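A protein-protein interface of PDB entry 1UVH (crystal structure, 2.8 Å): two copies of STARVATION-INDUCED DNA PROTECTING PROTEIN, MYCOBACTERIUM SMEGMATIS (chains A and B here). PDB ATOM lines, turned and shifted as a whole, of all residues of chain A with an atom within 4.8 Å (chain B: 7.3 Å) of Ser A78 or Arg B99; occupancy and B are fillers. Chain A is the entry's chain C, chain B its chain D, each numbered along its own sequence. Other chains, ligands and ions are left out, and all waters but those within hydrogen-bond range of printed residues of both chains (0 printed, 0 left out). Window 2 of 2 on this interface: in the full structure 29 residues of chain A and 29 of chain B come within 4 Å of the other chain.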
ATOM      1  N   GLN A  22      31.410 -14.767  14.764  1.00  0.00           N
ATOM      2  CA  GLN A  22      31.481 -15.590  15.963  1.00  0.00           C
ATOM      3  C   GLN A  22      32.030 -14.822  17.173  1.00  0.00           C
ATOM      4  O   GLN A  22      31.479 -14.925  18.259  1.00  0.00           O
ATOM      5  CB  GLN A  22      32.307 -16.847  15.736  1.00  0.00           C
ATOM      6  CG  GLN A  22      32.420 -17.714  17.004  1.00  0.00           C
ATOM      7  CD  GLN A  22      31.078 -18.077  17.630  1.00  0.00           C
ATOM      8  OE1 GLN A  22      30.406 -18.978  17.143  1.00  0.00           O
ATOM      9  NE2 GLN A  22      30.704 -17.402  18.709  1.00  0.00           N
ATOM     10  N   ILE A  72      26.523 -16.538  10.206  1.00  0.00           N
ATOM     11  CA  ILE A  72      27.574 -17.558  10.280  1.00  0.00           C
ATOM     12  C   ILE A  72      27.166 -18.813   9.555  1.00  0.00           C
ATOM     13  O   ILE A  72      27.883 -19.288   8.702  1.00  0.00           O
ATOM     14  CB  ILE A  72      27.875 -17.931  11.723  1.00  0.00           C
ATOM     15  CG1 ILE A  72      28.765 -16.889  12.367  1.00  0.00           C
ATOM     16  CG2 ILE A  72      28.541 -19.275  11.817  1.00  0.00           C
ATOM     17  CD1 ILE A  72      28.599 -16.828  13.856  1.00  0.00           C
ATOM     18  N   GLY A  76      28.530 -20.754   6.097  1.00  0.00           N
ATOM     19  CA  GLY A  76      28.918 -22.155   6.009  1.00  0.00           C
ATOM     20  C   GLY A  76      29.293 -22.733   7.373  1.00  0.00           C
ATOM     21  O   GLY A  76      28.894 -23.831   7.719  1.00  0.00           O
ATOM     22  N   LYS A  77      30.082 -21.998   8.148  1.00  0.00           N
ATOM     23  CA  LYS A  77      30.485 -22.443   9.469  1.00  0.00           C
ATOM     24  C   LYS A  77      29.295 -22.703  10.415  1.00  0.00           C
ATOM     25  O   LYS A  77      28.170 -22.266  10.147  1.00  0.00           O
ATOM     26  CB  LYS A  77      31.406 -21.396  10.091  1.00  0.00           C
ATOM     27  CG  LYS A  77      32.893 -21.545   9.715  1.00  0.00           C
ATOM     28  CD  LYS A  77      33.808 -21.077  10.906  1.00  0.00           C
ATOM     29  CE  LYS A  77      35.270 -21.405  10.699  1.00  0.00           C
ATOM     30  NZ  LYS A  77      35.697 -22.324  11.776  1.00  0.00           N
ATOM     31  N   SER A  78      29.577 -23.426  11.510  1.00  0.00           N
ATOM     32  CA  SER A  78      28.643 -23.572  12.623  1.00  0.00           C
ATOM     33  C   SER A  78      28.894 -22.521  13.695  1.00  0.00           C
ATOM     34  O   SER A  78      30.030 -22.340  14.137  1.00  0.00           O
ATOM     35  CB  SER A  78      28.757 -24.933  13.289  1.00  0.00           C
ATOM     36  OG  SER A  78      28.256 -24.872  14.624  1.00  0.00           O
ATOM     37  N   PRO A  79      27.834 -21.828  14.109  1.00  0.00           N
ATOM     38  CA  PRO A  79      27.897 -20.814  15.178  1.00  0.00           C
ATOM     39  C   PRO A  79      27.719 -21.377  16.569  1.00  0.00           C
ATOM     40  O   PRO A  79      27.094 -22.406  16.724  1.00  0.00           O
ATOM     41  CB  PRO A  79      26.695 -19.925  14.862  1.00  0.00           C
ATOM     42  CG  PRO A  79      25.718 -20.861  14.310  1.00  0.00           C
ATOM     43  CD  PRO A  79      26.484 -21.905  13.543  1.00  0.00           C
ATOM     44  N   LYS A  80      28.212 -20.670  17.565  1.00  0.00           N
ATOM     45  CA  LYS A  80      28.369 -21.261  18.879  1.00  0.00           C
ATOM     46  C   LYS A  80      27.826 -20.310  19.944  1.00  0.00           C
ATOM     47  O   LYS A  80      28.340 -19.196  20.096  1.00  0.00           O
ATOM     48  CB  LYS A  80      29.860 -21.632  19.113  1.00  0.00           C
ATOM     49  CG  LYS A  80      30.598 -22.238  17.869  1.00  0.00           C
ATOM     50  CD  LYS A  80      31.710 -23.276  18.210  1.00  0.00           C
ATOM     51  CE  LYS A  80      33.162 -22.699  18.230  1.00  0.00           C
ATOM     52  NZ  LYS A  80      34.134 -23.564  19.029  1.00  0.00           N
ATOM     53  N   HIS B  37      21.203 -21.838  20.738  1.00  0.00           N
ATOM     54  CA  HIS B  37      22.374 -22.521  20.134  1.00  0.00           C
ATOM     55  C   HIS B  37      21.947 -23.662  19.241  1.00  0.00           C
ATOM     56  O   HIS B  37      22.429 -23.794  18.096  1.00  0.00           O
ATOM     57  CB  HIS B  37      23.355 -23.095  21.175  1.00  0.00           C
ATOM     58  CG  HIS B  37      24.529 -23.796  20.538  1.00  0.00           C
ATOM     59  ND1 HIS B  37      24.749 -25.152  20.650  1.00  0.00           N
ATOM     60  CD2 HIS B  37      25.480 -23.335  19.690  1.00  0.00           C
ATOM     61  CE1 HIS B  37      25.797 -25.487  19.918  1.00  0.00           C
ATOM     62  NE2 HIS B  37      26.255 -24.402  19.326  1.00  0.00           N
ATOM     63  N   TRP B  40      19.892 -22.557  15.846  1.00  0.00           N
ATOM     64  CA  TRP B  40      20.566 -22.128  14.655  1.00  0.00           C
ATOM     65  C   TRP B  40      21.631 -23.142  14.226  1.00  0.00           C
ATOM     66  O   TRP B  40      22.186 -22.995  13.137  1.00  0.00           O
ATOM     67  CB  TRP B  40      21.032 -20.650  14.737  1.00  0.00           C
ATOM     68  CG  TRP B  40      21.806 -20.291  15.913  1.00  0.00           C
ATOM     69  CD1 TRP B  40      22.906 -20.932  16.367  1.00  0.00           C
ATOM     70  CD2 TRP B  40      21.583 -19.197  16.818  1.00  0.00           C
ATOM     71  NE1 TRP B  40      23.405 -20.305  17.490  1.00  0.00           N
ATOM     72  CE2 TRP B  40      22.609 -19.244  17.800  1.00  0.00           C
ATOM     73  CE3 TRP B  40      20.646 -18.180  16.896  1.00  0.00           C
ATOM     74  CZ2 TRP B  40      22.709 -18.341  18.854  1.00  0.00           C
ATOM     75  CZ3 TRP B  40      20.772 -17.252  17.961  1.00  0.00           C
ATOM     76  CH2 TRP B  40      21.797 -17.356  18.924  1.00  0.00           C
ATOM     77  N   ASN B  41      21.839 -24.208  15.014  1.00  0.00           N
ATOM     78  CA  ASN B  41      22.665 -25.376  14.597  1.00  0.00           C
ATOM     79  C   ASN B  41      21.923 -26.645  14.119  1.00  0.00           C
ATOM     80  O   ASN B  41      22.531 -27.618  13.646  1.00  0.00           O
ATOM     81  CB  ASN B  41      23.620 -25.766  15.714  1.00  0.00           C
ATOM     82  CG  ASN B  41      24.871 -24.935  15.691  1.00  0.00           C
ATOM     83  OD1 ASN B  41      25.044 -24.059  16.525  1.00  0.00           O
ATOM     84  ND2 ASN B  41      25.745 -25.184  14.714  1.00  0.00           N
ATOM     85  N   VAL B  42      20.611 -26.632  14.223  1.00  0.00           N
ATOM     86  CA  VAL B  42      19.804 -27.763  13.809  1.00  0.00           C
ATOM     87  C   VAL B  42      19.853 -27.872  12.273  1.00  0.00           C
ATOM     88  O   VAL B  42      20.356 -26.976  11.625  1.00  0.00           O
ATOM     89  CB  VAL B  42      18.394 -27.602  14.411  1.00  0.00           C
ATOM     90  CG1 VAL B  42      17.275 -27.661  13.360  1.00  0.00           C
ATOM     91  CG2 VAL B  42      18.199 -28.610  15.521  1.00  0.00           C
ATOM     92  N   VAL B  43      19.366 -28.973  11.700  1.00  0.00           N
ATOM     93  CA  VAL B  43      19.653 -29.297  10.291  1.00  0.00           C
ATOM     94  C   VAL B  43      19.004 -30.643   9.800  1.00  0.00           C
ATOM     95  O   VAL B  43      18.633 -31.522  10.590  1.00  0.00           O
ATOM     96  CB  VAL B  43      21.213 -29.269  10.067  1.00  0.00           C
ATOM     97  CG1 VAL B  43      21.832 -30.605  10.350  1.00  0.00           C
ATOM     98  CG2 VAL B  43      21.565 -28.779   8.694  1.00  0.00           C
ATOM     99  N   SER B  96      27.578 -29.604  24.398  1.00  0.00           N
ATOM    100  CA  SER B  96      28.677 -30.057  23.532  1.00  0.00           C
ATOM    101  C   SER B  96      28.317 -30.109  22.038  1.00  0.00           C
ATOM    102  O   SER B  96      29.190 -29.996  21.175  1.00  0.00           O
ATOM    103  CB  SER B  96      29.090 -31.465  23.964  1.00  0.00           C
ATOM    104  OG  SER B  96      28.032 -32.384  23.731  1.00  0.00           O
ATOM    105  N   VAL B  97      27.033 -30.285  21.753  1.00  0.00           N
ATOM    106  CA  VAL B  97      26.577 -30.596  20.399  1.00  0.00           C
ATOM    107  C   VAL B  97      26.627 -29.384  19.474  1.00  0.00           C
ATOM    108  O   VAL B  97      26.099 -28.332  19.777  1.00  0.00           O
ATOM    109  CB  VAL B  97      25.150 -31.131  20.373  1.00  0.00           C
ATOM    110  CG1 VAL B  97      24.948 -31.965  19.171  1.00  0.00           C
ATOM    111  CG2 VAL B  97      24.850 -31.910  21.602  1.00  0.00           C
ATOM    112  N   GLU B  98      27.260 -29.549  18.328  1.00  0.00           N
ATOM    113  CA  GLU B  98      27.506 -28.439  17.410  1.00  0.00           C
ATOM    114  C   GLU B  98      26.624 -28.660  16.129  1.00  0.00           C
ATOM    115  O   GLU B  98      25.641 -29.414  16.192  1.00  0.00           O
ATOM    116  CB  GLU B  98      29.031 -28.338  17.145  1.00  0.00           C
ATOM    117  CG  GLU B  98      29.791 -27.296  17.981  1.00  0.00           C
ATOM    118  CD  GLU B  98      30.515 -26.257  17.106  1.00  0.00           C
ATOM    119  OE1 GLU B  98      31.593 -26.579  16.539  1.00  0.00           O
ATOM    120  OE2 GLU B  98      30.003 -25.119  16.960  1.00  0.00           O
ATOM    121  N   ARG B  99      26.912 -28.011  14.997  1.00  0.00           N
ATOM    122  CA  ARG B  99      26.046 -28.234  13.853  1.00  0.00           C
ATOM    123  C   ARG B  99      25.732 -29.710  13.809  1.00  0.00           C
ATOM    124  O   ARG B  99      26.627 -30.533  13.929  1.00  0.00           O
ATOM    125  CB  ARG B  99      26.692 -27.847  12.550  1.00  0.00           C
ATOM    126  CG  ARG B  99      26.278 -28.748  11.381  1.00  0.00           C
ATOM    127  CD  ARG B  99      27.289 -28.753  10.275  1.00  0.00           C
ATOM    128  NE  ARG B  99      27.338 -27.420   9.686  1.00  0.00           N
ATOM    129  CZ  ARG B  99      27.324 -27.161   8.386  1.00  0.00           C
ATOM    130  NH1 ARG B  99      27.301 -28.140   7.481  1.00  0.00           N
ATOM    131  NH2 ARG B  99      27.350 -25.901   7.983  1.00  0.00           N
ATOM    132  N   ASP B 100      24.472 -30.055  13.621  1.00  0.00           N
ATOM    133  CA  ASP B 100      24.064 -31.458  13.676  1.00  0.00           C
ATOM    134  C   ASP B 100      22.558 -31.599  13.423  1.00  0.00           C
ATOM    135  O   ASP B 100      21.818 -30.614  13.439  1.00  0.00           O
ATOM    136  CB  ASP B 100      24.435 -32.078  15.033  1.00  0.00           C
ATOM    137  CG  ASP B 100      24.838 -33.526  14.921  1.00  0.00           C
ATOM    138  OD1 ASP B 100      24.078 -34.290  14.303  1.00  0.00           O
ATOM    139  OD2 ASP B 100      25.878 -33.996  15.436  1.00  0.00           O
ATOM    140  N   THR B 101      22.120 -32.829  13.171  1.00  0.00           N
ATOM    141  CA  THR B 101      20.749 -33.094  12.781  1.00  0.00           C
ATOM    142  C   THR B 101      19.807 -32.736  13.895  1.00  0.00           C
ATOM    143  O   THR B 101      20.221 -32.390  15.001  1.00  0.00           O
ATOM    144  CB  THR B 101      20.546 -34.576  12.432  1.00  0.00           C
ATOM    145  OG1 THR B 101      21.166 -35.383  13.438  1.00  0.00           O
ATOM    146  CG2 THR B 101      21.252 -34.943  11.131  1.00  0.00           C
ATOM    147  N   ALA B 104      19.689 -35.627  16.545  1.00  0.00           N
ATOM    148  CA  ALA B 104      20.860 -35.534  17.408  1.00  0.00           C
ATOM    149  C   ALA B 104      20.621 -34.537  18.534  1.00  0.00           C
ATOM    150  O   ALA B 104      20.655 -34.876  19.736  1.00  0.00           O
ATOM    151  CB  ALA B 104      22.065 -35.105  16.591  1.00  0.00           C
ATOM    152  N   HIS B 105      20.387 -33.294  18.109  1.00  0.00           N
ATOM    153  CA  HIS B 105      20.146 -32.144  18.982  1.00  0.00           C
ATOM    154  C   HIS B 105      18.956 -32.313  19.933  1.00  0.00           C
ATOM    155  O   HIS B 105      18.978 -31.821  21.050  1.00  0.00           O
ATOM    156  CB  HIS B 105      19.894 -30.923  18.113  1.00  0.00           C
ATOM    157  CG  HIS B 105      21.132 -30.231  17.662  1.00  0.00           C
ATOM    158  ND1 HIS B 105      22.078 -29.761  18.542  1.00  0.00           N
ATOM    159  CD2 HIS B 105      21.541 -29.854  16.427  1.00  0.00           C
ATOM    160  CE1 HIS B 105      23.040 -29.157  17.864  1.00  0.00           C
ATOM    161  NE2 HIS B 105      22.733 -29.186  16.578  1.00  0.00           N
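O of Gly A76 lies within hydrogen-bond range of NH2 of Arg B99 (2.6 Å). The side-chain amide oxygen (OD1) of Asn B41 lies close to the backbone carbonyl oxygen (O) of Pro A79, 2.6 Å away. N of Arg B99 is in hydrogen-bond range of OG of Ser A78 (3.4 Å). OE2 of Glu B98 is in hydrogen-bond range of OG of Ser A78 (2.9 Å). A ring nitrogen (NE2) of His B37 is in hydrogen-bond range of the backbone carbonyl oxygen of Pro A79 (3.4 Å). ND2 of Asn B41 is in hydrogen-bond range of OG of Ser A78.
The side-chain amide nitrogen of Asn B41 lies close to the backbone NH of Arg B99, at 3.1 Å. NE2 of His B105 sits at hydrogen-bond distance from O of Asn B41 (3.3 Å). The backbone carbonyl oxygen (O) of Asn B41 lies within hydrogen-bond range of the backbone NH (N) of Asp B100 (3.1 Å). The side-chain amide oxygen (OE1) of Gln A22 lies within hydrogen-bond range of the backbone NH (N) of Lys A80 (2.8 Å). The side-chain amide oxygen of Asn B41 lies close to the backbone carbonyl oxygen of His B37, 3.1 Å away. NE2 of His B105 is in hydrogen-bond range of O of Glu B98, 2.9 Å away.
Among the printed residues, merely in contact across the chains: Pro A79 with Trp B40 (3.5 Å), Pro A79 with Glu B98 (3.98 Å), Lys A80 with His B37 (3.6 Å) and Lys A80 with Glu B98 (2.8 Å).
Ser A78 touches just these residues of chain B: Asn B41 (2.5 Å), Glu B98 (2.9 Å) and Arg B99 (3.4 Å). Printed residues of chain B within 4 Å of Pro A79: His B37 (3.4 Å), Trp B40 (3.5 Å), Asn B41 (2.6 Å) and Glu B98 (3.98 Å). Of the printed residues of chain B, Lys A80 touches His B37 (3.6 Å) and Glu B98 (2.8 Å). Of the printed residues of chain A, His B37 touches Pro A79 and Lys A80. Of the printed residues of chain A, Trp B40 touches Pro A79. Printed residues of chain A within 4 Å of Asn B41: Ser A78 and Pro A79. Val B43 touches none of the printed residues of chain A. Of the printed residues of chain A, Arg B99 touches Gly A76 (2.6 Å) and Ser A78 (3.4 Å). The nearest residue of chain B that does not touch Ser A78 is His B37 (5.1 Å). The nearest residue of chain A that does not touch Arg B99 is Lys A77 (4.3 Å).
Hydrophobic or aromatic side chains of chain A within 4 Å of the printed part of chain B: Pro A79. Of the 13 printed residues of chain B, 5 touch a printed residue of chain A.
No position is printed for both chains.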
